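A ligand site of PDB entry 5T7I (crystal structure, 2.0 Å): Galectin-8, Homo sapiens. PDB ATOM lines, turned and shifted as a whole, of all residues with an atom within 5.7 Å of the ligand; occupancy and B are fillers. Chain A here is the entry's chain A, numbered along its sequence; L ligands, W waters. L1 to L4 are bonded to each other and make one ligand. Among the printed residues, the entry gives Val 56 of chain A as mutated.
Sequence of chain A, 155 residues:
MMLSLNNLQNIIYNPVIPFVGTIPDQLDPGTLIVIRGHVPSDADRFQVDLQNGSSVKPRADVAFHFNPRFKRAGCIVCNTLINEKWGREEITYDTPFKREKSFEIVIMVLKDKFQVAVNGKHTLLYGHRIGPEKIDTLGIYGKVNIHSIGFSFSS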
ATOM      1  N   PRO A  18      -3.653  -8.656 -11.849  1.00  0.00           N
ATOM      2  CA  PRO A  18      -4.953  -8.790 -12.511  1.00  0.00           C
ATOM      3  C   PRO A  18      -5.004  -8.217 -13.930  1.00  0.00           C
ATOM      4  O   PRO A  18      -4.489  -7.134 -14.192  1.00  0.00           O
ATOM      5  CB  PRO A  18      -5.919  -8.042 -11.566  1.00  0.00           C
ATOM      6  CG  PRO A  18      -5.060  -7.057 -10.846  1.00  0.00           C
ATOM      7  CD  PRO A  18      -3.722  -7.734 -10.698  1.00  0.00           C
ATOM      8  N   ARG A  45      -6.976 -19.945  -5.132  1.00  0.00           N
ATOM      9  CA  ARG A  45      -7.965 -19.856  -6.210  1.00  0.00           C
ATOM     10  C   ARG A  45      -7.550 -18.865  -7.296  1.00  0.00           C
ATOM     11  O   ARG A  45      -6.715 -18.000  -7.065  1.00  0.00           O
ATOM     12  CB  ARG A  45      -9.316 -19.474  -5.632  1.00  0.00           C
ATOM     13  CG  ARG A  45      -9.255 -18.440  -4.508  1.00  0.00           C
ATOM     14  CD  ARG A  45     -10.651 -17.943  -4.166  1.00  0.00           C
ATOM     15  NE  ARG A  45     -11.179 -17.069  -5.218  1.00  0.00           N
ATOM     16  CZ  ARG A  45     -12.481 -16.822  -5.433  1.00  0.00           C
ATOM     17  NH1 ARG A  45     -13.431 -17.373  -4.698  1.00  0.00           N
ATOM     18  NH2 ARG A  45     -12.816 -16.005  -6.420  1.00  0.00           N
ATOM     19  N   GLN A  47      -9.602 -16.915 -11.072  1.00  0.00           N
ATOM     20  CA  GLN A  47     -10.825 -16.896 -11.840  1.00  0.00           C
ATOM     21  C   GLN A  47     -10.683 -16.180 -13.154  1.00  0.00           C
ATOM     22  O   GLN A  47      -9.908 -15.235 -13.282  1.00  0.00           O
ATOM     23  CB  GLN A  47     -11.995 -16.308 -11.039  1.00  0.00           C
ATOM     24  CG  GLN A  47     -11.809 -14.872 -10.587  1.00  0.00           C
ATOM     25  CD  GLN A  47     -11.322 -14.724  -9.169  1.00  0.00           C
ATOM     26  OE1 GLN A  47     -10.629 -15.584  -8.629  1.00  0.00           O
ATOM     27  NE2 GLN A  47     -11.686 -13.601  -8.550  1.00  0.00           N
ATOM     28  N   ASP A  49     -13.234 -14.318 -15.711  1.00  0.00           N
ATOM     29  CA  ASP A  49     -14.541 -13.657 -15.729  1.00  0.00           C
ATOM     30  C   ASP A  49     -14.833 -13.099 -17.111  1.00  0.00           C
ATOM     31  O   ASP A  49     -14.033 -12.357 -17.634  1.00  0.00           O
ATOM     32  CB  ASP A  49     -14.576 -12.491 -14.715  1.00  0.00           C
ATOM     33  CG  ASP A  49     -14.600 -12.957 -13.266  1.00  0.00           C
ATOM     34  OD1 ASP A  49     -14.775 -14.159 -13.030  1.00  0.00           O
ATOM     35  OD2 ASP A  49     -14.464 -12.113 -12.354  1.00  0.00           O
ATOM     36  N   GLN A  51     -17.090 -10.620 -18.781  1.00  0.00           N
ATOM     37  CA  GLN A  51     -17.796  -9.492 -18.176  1.00  0.00           C
ATOM     38  C   GLN A  51     -18.540  -8.639 -19.210  1.00  0.00           C
ATOM     39  O   GLN A  51     -18.123  -8.532 -20.378  1.00  0.00           O
ATOM     40  CB  GLN A  51     -16.814  -8.583 -17.405  1.00  0.00           C
ATOM     41  CG  GLN A  51     -15.992  -9.278 -16.338  1.00  0.00           C
ATOM     42  CD  GLN A  51     -14.979  -8.376 -15.631  1.00  0.00           C
ATOM     43  OE1 GLN A  51     -14.161  -8.865 -14.851  1.00  0.00           O
ATOM     44  NE2 GLN A  51     -15.022  -7.071 -15.906  1.00  0.00           N
ATOM     45  N   SER A  55     -16.580  -1.776 -15.412  1.00  0.00           N
ATOM     46  CA  SER A  55     -16.953  -1.006 -14.232  1.00  0.00           C
ATOM     47  C   SER A  55     -16.637  -1.785 -12.954  1.00  0.00           C
ATOM     48  O   SER A  55     -16.741  -3.026 -12.923  1.00  0.00           O
ATOM     49  CB  SER A  55     -18.447  -0.629 -14.288  1.00  0.00           C
ATOM     50  OG  SER A  55     -18.859   0.077 -13.132  1.00  0.00           O
ATOM     51  N   VAL A  56     -16.204  -1.060 -11.931  1.00  0.00           N
ATOM     52  CA  VAL A  56     -15.934  -1.598 -10.585  1.00  0.00           C
ATOM     53  C   VAL A  56     -16.906  -1.100  -9.508  1.00  0.00           C
ATOM     54  O   VAL A  56     -16.929  -1.649  -8.393  1.00  0.00           O
ATOM     55  CB  VAL A  56     -14.465  -1.343 -10.120  1.00  0.00           C
ATOM     56  CG1 VAL A  56     -13.494  -2.099 -11.006  1.00  0.00           C
ATOM     57  CG2 VAL A  56     -14.123   0.144 -10.062  1.00  0.00           C
ATOM     58  N   ARG A  59     -19.924  -3.124  -9.628  1.00  0.00           N
ATOM     59  CA  ARG A  59     -19.114  -4.209 -10.219  1.00  0.00           C
ATOM     60  C   ARG A  59     -19.757  -4.682 -11.509  1.00  0.00           C
ATOM     61  O   ARG A  59     -20.958  -5.029 -11.508  1.00  0.00           O
ATOM     62  CB  ARG A  59     -18.993  -5.406  -9.272  1.00  0.00           C
ATOM     63  CG  ARG A  59     -18.166  -5.172  -8.022  1.00  0.00           C
ATOM     64  CD  ARG A  59     -16.693  -5.069  -8.335  1.00  0.00           C
ATOM     65  NE  ARG A  59     -15.916  -4.753  -7.143  1.00  0.00           N
ATOM     66  CZ  ARG A  59     -14.643  -4.351  -7.132  1.00  0.00           C
ATOM     67  NH1 ARG A  59     -13.956  -4.223  -8.268  1.00  0.00           N
ATOM     68  NH2 ARG A  59     -14.052  -4.093  -5.974  1.00  0.00           N
ATOM     69  N   VAL A  62     -20.989 -10.256 -14.438  1.00  0.00           N
ATOM     70  CA  VAL A  62     -20.126 -11.335 -14.894  1.00  0.00           C
ATOM     71  C   VAL A  62     -21.021 -12.454 -15.424  1.00  0.00           C
ATOM     72  O   VAL A  62     -21.654 -13.197 -14.646  1.00  0.00           O
ATOM     73  CB  VAL A  62     -19.211 -11.858 -13.763  1.00  0.00           C
ATOM     74  CG1 VAL A  62     -18.328 -12.990 -14.310  1.00  0.00           C
ATOM     75  CG2 VAL A  62     -18.368 -10.720 -13.161  1.00  0.00           C
ATOM     76  N   HIS A  65     -18.370 -16.730 -14.528  1.00  0.00           N
ATOM     77  CA  HIS A  65     -17.292 -16.739 -13.541  1.00  0.00           C
ATOM     78  C   HIS A  65     -16.817 -18.189 -13.451  1.00  0.00           C
ATOM     79  O   HIS A  65     -17.568 -19.068 -13.028  1.00  0.00           O
ATOM     80  CB  HIS A  65     -17.839 -16.185 -12.228  1.00  0.00           C
ATOM     81  CG  HIS A  65     -16.913 -16.277 -11.050  1.00  0.00           C
ATOM     82  ND1 HIS A  65     -15.840 -15.434 -10.856  1.00  0.00           N
ATOM     83  CD2 HIS A  65     -16.966 -17.063  -9.941  1.00  0.00           C
ATOM     84  CE1 HIS A  65     -15.244 -15.716  -9.712  1.00  0.00           C
ATOM     85  NE2 HIS A  65     -15.924 -16.686  -9.123  1.00  0.00           N
ATOM     86  N   ASN A  67     -14.027 -20.457 -11.851  1.00  0.00           N
ATOM     87  CA  ASN A  67     -13.267 -20.205 -10.615  1.00  0.00           C
ATOM     88  C   ASN A  67     -12.663 -21.493 -10.023  1.00  0.00           C
ATOM     89  O   ASN A  67     -13.252 -22.087  -9.115  1.00  0.00           O
ATOM     90  CB  ASN A  67     -14.198 -19.488  -9.621  1.00  0.00           C
ATOM     91  CG  ASN A  67     -13.595 -19.245  -8.230  1.00  0.00           C
ATOM     92  OD1 ASN A  67     -14.322 -19.309  -7.240  1.00  0.00           O
ATOM     93  ND2 ASN A  67     -12.294 -19.006  -8.141  1.00  0.00           N
ATOM     94  N   ARG A  69     -10.663 -23.643  -7.541  1.00  0.00           N
ATOM     95  CA  ARG A  69     -10.257 -23.555  -6.138  1.00  0.00           C
ATOM     96  C   ARG A  69      -9.389 -24.765  -5.761  1.00  0.00           C
ATOM     97  O   ARG A  69      -9.634 -25.869  -6.246  1.00  0.00           O
ATOM     98  CB  ARG A  69     -11.499 -23.484  -5.258  1.00  0.00           C
ATOM     99  CG  ARG A  69     -12.383 -22.305  -5.580  1.00  0.00           C
ATOM    100  CD  ARG A  69     -13.545 -22.155  -4.619  1.00  0.00           C
ATOM    101  NE  ARG A  69     -14.350 -20.997  -4.955  1.00  0.00           N
ATOM    102  CZ  ARG A  69     -15.444 -20.608  -4.323  1.00  0.00           C
ATOM    103  NH1 ARG A  69     -15.899 -21.283  -3.264  1.00  0.00           N
ATOM    104  NH2 ARG A  69     -16.093 -19.524  -4.752  1.00  0.00           N
ATOM    105  N   CME A  75     -11.885 -27.935  -6.613  1.00  0.00           N
ATOM    106  CA  CME A  75     -13.104 -27.955  -7.425  1.00  0.00           C
ATOM    107  CB  CME A  75     -14.349 -27.819  -6.539  1.00  0.00           C
ATOM    108  SG  CME A  75     -14.517 -26.230  -5.777  1.00  0.00           S
ATOM    109  SD  CME A  75     -13.989 -26.378  -3.852  1.00  0.00           S
ATOM    110  CE  CME A  75     -15.435 -27.042  -3.067  1.00  0.00           C
ATOM    111  CZ  CME A  75     -16.595 -26.033  -2.985  1.00  0.00           C
ATOM    112  OH  CME A  75     -16.222 -24.860  -2.252  1.00  0.00           O
ATOM    113  C   CME A  75     -12.995 -26.798  -8.393  1.00  0.00           C
ATOM    114  O   CME A  75     -12.045 -26.025  -8.340  1.00  0.00           O
ATOM    115  N   VAL A  77     -15.706 -23.687  -9.299  1.00  0.00           N
ATOM    116  CA  VAL A  77     -17.001 -23.033  -9.126  1.00  0.00           C
ATOM    117  C   VAL A  77     -17.329 -22.167 -10.322  1.00  0.00           C
ATOM    118  O   VAL A  77     -16.523 -21.336 -10.752  1.00  0.00           O
ATOM    119  CB  VAL A  77     -17.031 -22.192  -7.836  1.00  0.00           C
ATOM    120  CG1 VAL A  77     -18.341 -21.403  -7.733  1.00  0.00           C
ATOM    121  CG2 VAL A  77     -16.858 -23.098  -6.624  1.00  0.00           C
ATOM    122  N   CYS A  78     -18.517 -22.349 -10.887  1.00  0.00           N
ATOM    123  CA  CYS A  78     -19.033 -21.442 -11.894  1.00  0.00           C
ATOM    124  C   CYS A  78     -20.280 -20.700 -11.368  1.00  0.00           C
ATOM    125  O   CYS A  78     -21.097 -21.263 -10.640  1.00  0.00           O
ATOM    126  CB  CYS A  78     -19.305 -22.180 -13.201  1.00  0.00           C
ATOM    127  SG  CYS A  78     -17.835 -22.926 -13.936  1.00  0.00           S
ATOM    128  N   ASN A  79     -20.402 -19.429 -11.731  1.00  0.00           N
ATOM    129  CA  ASN A  79     -21.544 -18.634 -11.324  1.00  0.00           C
ATOM    130  C   ASN A  79     -21.664 -17.417 -12.241  1.00  0.00           C
ATOM    131  O   ASN A  79     -20.849 -17.240 -13.158  1.00  0.00           O
ATOM    132  CB  ASN A  79     -21.416 -18.212  -9.845  1.00  0.00           C
ATOM    133  CG  ASN A  79     -22.753 -18.019  -9.148  1.00  0.00           C
ATOM    134  OD1 ASN A  79     -23.817 -17.979  -9.793  1.00  0.00           O
ATOM    135  ND2 ASN A  79     -22.724 -17.945  -7.826  1.00  0.00           N
ATOM    136  N   TRP A  86     -24.480 -12.596  -6.629  1.00  0.00           N
ATOM    137  CA  TRP A  86     -24.167 -13.918  -7.168  1.00  0.00           C
ATOM    138  C   TRP A  86     -25.425 -14.784  -7.270  1.00  0.00           C
ATOM    139  O   TRP A  86     -26.308 -14.700  -6.412  1.00  0.00           O
ATOM    140  CB  TRP A  86     -23.138 -14.602  -6.260  1.00  0.00           C
ATOM    141  CG  TRP A  86     -21.785 -14.001  -6.400  1.00  0.00           C
ATOM    142  CD1 TRP A  86     -21.102 -13.258  -5.473  1.00  0.00           C
ATOM    143  CD2 TRP A  86     -20.943 -14.059  -7.554  1.00  0.00           C
ATOM    144  NE1 TRP A  86     -19.898 -12.865  -5.968  1.00  0.00           N
ATOM    145  CE2 TRP A  86     -19.770 -13.336  -7.252  1.00  0.00           C
ATOM    146  CE3 TRP A  86     -21.060 -14.664  -8.829  1.00  0.00           C
ATOM    147  CZ2 TRP A  86     -18.712 -13.193  -8.170  1.00  0.00           C
ATOM    148  CZ3 TRP A  86     -19.986 -14.528  -9.746  1.00  0.00           C
ATOM    149  CH2 TRP A  86     -18.834 -13.791  -9.413  1.00  0.00           C
ATOM    150  N   GLY A  87     -25.510 -15.571  -8.328  1.00  0.00           N
ATOM    151  CA  GLY A  87     -26.611 -16.495  -8.518  1.00  0.00           C
ATOM    152  C   GLY A  87     -26.277 -17.798  -7.817  1.00  0.00           C
ATOM    153  O   GLY A  87     -25.454 -17.816  -6.946  1.00  0.00           O
ATOM    154  N   GLU A  89     -24.471 -21.238  -7.386  1.00  0.00           N
ATOM    155  CA  GLU A  89     -23.210 -21.817  -7.822  1.00  0.00           C
ATOM    156  C   GLU A  89     -23.409 -23.154  -8.532  1.00  0.00           C
ATOM    157  O   GLU A  89     -24.320 -23.915  -8.191  1.00  0.00           O
ATOM    158  CB  GLU A  89     -22.275 -22.007  -6.646  1.00  0.00           C
ATOM    159  CG  GLU A  89     -21.701 -20.699  -6.145  1.00  0.00           C
ATOM    160  CD  GLU A  89     -20.705 -20.870  -5.026  1.00  0.00           C
ATOM    161  OE1 GLU A  89     -20.607 -21.983  -4.504  1.00  0.00           O
ATOM    162  OE2 GLU A  89     -20.022 -19.890  -4.680  1.00  0.00           O
ATOM    163  N   TYR A 141      -8.135 -13.045 -12.739  1.00  0.00           N
ATOM    164  CA  TYR A 141      -7.767 -12.623 -11.394  1.00  0.00           C
ATOM    165  C   TYR A 141      -7.333 -13.756 -10.522  1.00  0.00           C
ATOM    166  O   TYR A 141      -7.684 -14.929 -10.739  1.00  0.00           O
ATOM    167  CB  TYR A 141      -8.939 -11.951 -10.709  1.00  0.00           C
ATOM    168  CG  TYR A 141      -9.696 -10.972 -11.563  1.00  0.00           C
ATOM    169  CD1 TYR A 141      -9.147  -9.741 -11.881  1.00  0.00           C
ATOM    170  CD2 TYR A 141     -10.979 -11.263 -12.041  1.00  0.00           C
ATOM    171  CE1 TYR A 141      -9.838  -8.815 -12.642  1.00  0.00           C
ATOM    172  CE2 TYR A 141     -11.678 -10.342 -12.805  1.00  0.00           C
ATOM    173  CZ  TYR A 141     -11.096  -9.121 -13.097  1.00  0.00           C
ATOM    174  OH  TYR A 141     -11.766  -8.204 -13.865  1.00  0.00           O
ATOM    175  N   GLY A 142      -6.588 -13.371  -9.471  1.00  0.00           N
ATOM    176  CA  GLY A 142      -6.157 -14.282  -8.430  1.00  0.00           C
ATOM    177  C   GLY A 142      -4.767 -14.840  -8.672  1.00  0.00           C
ATOM    178  O   GLY A 142      -3.963 -14.266  -9.413  1.00  0.00           O
HETATM  179  C1  LIG L   1     -19.870 -20.078  -0.883  1.00  0.00           C
HETATM  180  C2  LIG L   1     -18.681 -19.355  -1.547  1.00  0.00           C
HETATM  181  C3  LIG L   1     -19.007 -17.891  -1.839  1.00  0.00           C
HETATM  182  C4  LIG L   1     -19.606 -17.201  -0.596  1.00  0.00           C
HETATM  183  C5  LIG L   1     -20.004 -15.729  -0.784  1.00  0.00           C
HETATM  184  C6  LIG L   1     -20.448 -19.249   0.260  1.00  0.00           C
HETATM  185  O1  LIG L   1     -21.647 -19.859   0.726  1.00  0.00           O
HETATM  186  O2  LIG L   1     -19.418 -21.334  -0.356  1.00  0.00           O
HETATM  187  O3  LIG L   1     -18.320 -20.052  -2.742  1.00  0.00           O
HETATM  188  O4  LIG L   1     -17.789 -17.244  -2.256  1.00  0.00           O
HETATM  189  O5  LIG L   1     -20.781 -17.942  -0.210  1.00  0.00           O
HETATM  190  O6  LIG L   1     -20.925 -15.572  -1.886  1.00  0.00           O
HETATM  191  C1  LG2 L   2     -17.922 -16.400  -3.414  1.00  0.00           C
HETATM  192  C2  LG2 L   2     -16.579 -15.700  -3.642  1.00  0.00           C
HETATM  193  C3  LG2 L   2     -16.607 -14.942  -4.962  1.00  0.00           C
HETATM  194  C4  LG2 L   2     -17.051 -15.847  -6.118  1.00  0.00           C
HETATM  195  C5  LG2 L   2     -18.403 -16.477  -5.760  1.00  0.00           C
HETATM  196  C6  LG2 L   2     -18.959 -17.398  -6.830  1.00  0.00           C
HETATM  197  O1  LG2 L   2     -16.269 -14.756  -2.606  1.00  0.00           O
HETATM  198  O2  LG2 L   2     -15.327 -14.333  -5.205  1.00  0.00           O
HETATM  199  O3  LG2 L   2     -16.072 -16.857  -6.359  1.00  0.00           O
HETATM  200  O4  LG2 L   2     -18.258 -17.222  -4.534  1.00  0.00           O
HETATM  201  O5  LG2 L   2     -20.166 -17.992  -6.338  1.00  0.00           O
HETATM  202  C1  LG3 L   3     -15.100 -13.117  -5.707  1.00  0.00           C
HETATM  203  C2  LG3 L   3     -13.914 -12.398  -5.099  1.00  0.00           C
HETATM  204  C3  LG3 L   3     -13.773 -11.012  -5.697  1.00  0.00           C
HETATM  205  C4  LG3 L   3     -13.906 -11.018  -7.222  1.00  0.00           C
HETATM  206  C5  LG3 L   3     -15.122 -11.817  -7.674  1.00  0.00           C
HETATM  207  C6  LG3 L   3     -15.303 -11.861  -9.176  1.00  0.00           C
HETATM  208  C7  LG3 L   3     -13.241 -13.020  -2.815  1.00  0.00           C
HETATM  209  C8  LG3 L   3     -13.481 -12.875  -1.332  1.00  0.00           C
HETATM  210  N1  LG3 L   3     -14.035 -12.332  -3.642  1.00  0.00           N
HETATM  211  O1  LG3 L   3     -12.480 -10.520  -5.352  1.00  0.00           O
HETATM  212  O2  LG3 L   3     -14.104  -9.671  -7.658  1.00  0.00           O
HETATM  213  O3  LG3 L   3     -15.008 -13.129  -7.143  1.00  0.00           O
HETATM  214  O4  LG3 L   3     -14.216 -12.492  -9.834  1.00  0.00           O
HETATM  215  O5  LG3 L   3     -12.354 -13.737  -3.223  1.00  0.00           O
HETATM  216  C1  LG4 L   4     -13.183  -9.298  -8.668  1.00  0.00           C
HETATM  217  C2  LG4 L   4     -13.681  -7.956  -9.175  1.00  0.00           C
HETATM  218  C3  LG4 L   4     -12.669  -7.330 -10.107  1.00  0.00           C
HETATM  219  C4  LG4 L   4     -11.293  -7.300  -9.451  1.00  0.00           C
HETATM  220  C5  LG4 L   4     -10.906  -8.708  -9.028  1.00  0.00           C
HETATM  221  C6  LG4 L   4      -9.526  -8.727  -8.372  1.00  0.00           C
HETATM  222  O1  LG4 L   4     -14.949  -8.087  -9.829  1.00  0.00           O
HETATM  223  O2  LG4 L   4     -13.075  -6.000 -10.432  1.00  0.00           O
HETATM  224  O3  LG4 L   4     -11.310  -6.447  -8.299  1.00  0.00           O
HETATM  225  O4  LG4 L   4     -11.868  -9.218  -8.113  1.00  0.00           O
HETATM  226  O5  LG4 L   4      -9.247 -10.063  -7.939  1.00  0.00           O
HETATM  227  O   HOH W   1     -17.325  -7.681 -11.764  1.00  0.00           O
HETATM  228  O   HOH W   2     -12.579 -11.943   1.637  1.00  0.00           O
HETATM  229  O   HOH W   3     -17.266  -8.670  -8.780  1.00  0.00           O
HETATM  230  O   HOH W   4     -15.359  -5.399 -11.646  1.00  0.00           O
HETATM  231  O   HOH W   5      -6.049 -10.457  -8.886  1.00  0.00           O
HETATM  232  O   HOH W   6     -19.131 -23.002  -2.403  1.00  0.00           O
HETATM  233  O   HOH W   7     -12.440  -7.579  -5.782  1.00  0.00           O
HETATM  234  O   HOH W   8     -17.969 -12.506  -2.335  1.00  0.00           O
HETATM  235  O   HOH W   9     -22.215 -13.364  -2.103  1.00  0.00           O
HETATM  236  O   HOH W  10     -10.806  -3.126  -8.753  1.00  0.00           O
HETATM  237  O   HOH W  11     -15.202  -9.431 -12.346  1.00  0.00           O
HETATM  238  O   HOH W  12     -10.427 -11.848  -6.219  1.00  0.00           O
HETATM  239  O   HOH W  13     -21.791 -16.961  -4.229  1.00  0.00           O
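OE2 of Glu 89 is in hydrogen-bond range of O5 of LG2 L2.
OD2 of Asp 49 lies within hydrogen-bond range of O4 of LG3 L3 (2.6 Å).
An oxygen (O3) of LIG L1 is in hydrogen-bond range of the guanidinium group of Arg 69 (2.8 Å).
A ring nitrogen (NE2) of His 65 is in hydrogen-bond range of an oxygen (O3) of LG2 L2, 2.8 Å away.
An oxygen (O2) of LG4 L4 lies within hydrogen-bond range of the guanidinium group (NH1) of Arg 59 (2.9 Å).
ND2 of Asn 79 is in hydrogen-bond range of O5 of LG2 L2 (3.0 Å).
NE2 of Gln 47 sits at hydrogen-bond distance from O4 of LG3 L3, 3.0 Å away.
OD1 of Asn 67 is in hydrogen-bond range of O3 of LG2 L2 (3.1 Å).
An oxygen (O3) of LG2 L2 sits at hydrogen-bond distance from the guanidinium group (NH1) of Arg 45.
The side-chain carboxylate (OD1) of Asp 49 sits at hydrogen-bond distance from a ring nitrogen (ND1) of His 65, at 2.7 Å.
The guanidinium group (NE) of Arg 69 lies within hydrogen-bond range of the side-chain amide oxygen (OD1) of Asn 67, 2.8 Å away.
N of Arg 69 is in hydrogen-bond range of O of CME 75, at 2.9 Å.
N of His 65 sits at hydrogen-bond distance from O of Asn 79, at 2.9 Å.
The guanidinium group (NE) of Arg 59 sits close to the backbone carbonyl oxygen (O) of Val 56.
The side-chain amide nitrogen (ND2) of Asn 79 is in hydrogen-bond range of the backbone carbonyl oxygen (O) of Gly 87.
OD1 of Asn 67 is in hydrogen-bond range of NH1 of Arg 45.
The side-chain amide oxygen of Gln 51 is in hydrogen-bond range of the side-chain hydroxyl of Tyr 141.
Residues that only touch the ligand: Tyr 141 (3.4 Å), Trp 86 (3.7 Å) and Val 56 (3.97 Å).
Hydrophobic or aromatic side chains within 4 Å of the ligand: Val 56, His 65, Trp 86 and Tyr 141.
Within 4 Å of the ligand: Arg 45, Gln 47, Asp 49, Val 56, Arg 59, His 65, Asn 67, Arg 69, Asn 79, Trp 86, Glu 89 and Tyr 141.
Water W4 bridges an oxygen (O2) of LG4 L4 (2.7 Å) and the backbone carbonyl oxygen of Ser 55 (3.0 Å).
Water W6 lies within hydrogen-bond range of O2 of LIG L1, OE1 of Glu 89 and OH of CME 75.
Water W13 lies within hydrogen-bond range of an oxygen (O5) of LG2 L2 and the side-chain carboxylate (OE2) of Glu 89.
Water W11 lies within hydrogen-bond range of the side-chain amide oxygen of Gln 51 (2.8 Å), the side-chain carboxylate of Asp 49 (2.8 Å) and an oxygen (O1) of LG4 L4 (2.9 Å).
Water W5 bridges the backbone NH (N) of Gly 142 and an oxygen (O5) of LG4 L4.
Water W10 lies within hydrogen-bond range of NH1 of Arg 59 (3.4 Å) and O3 of LG4 L4 (3.4 Å).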
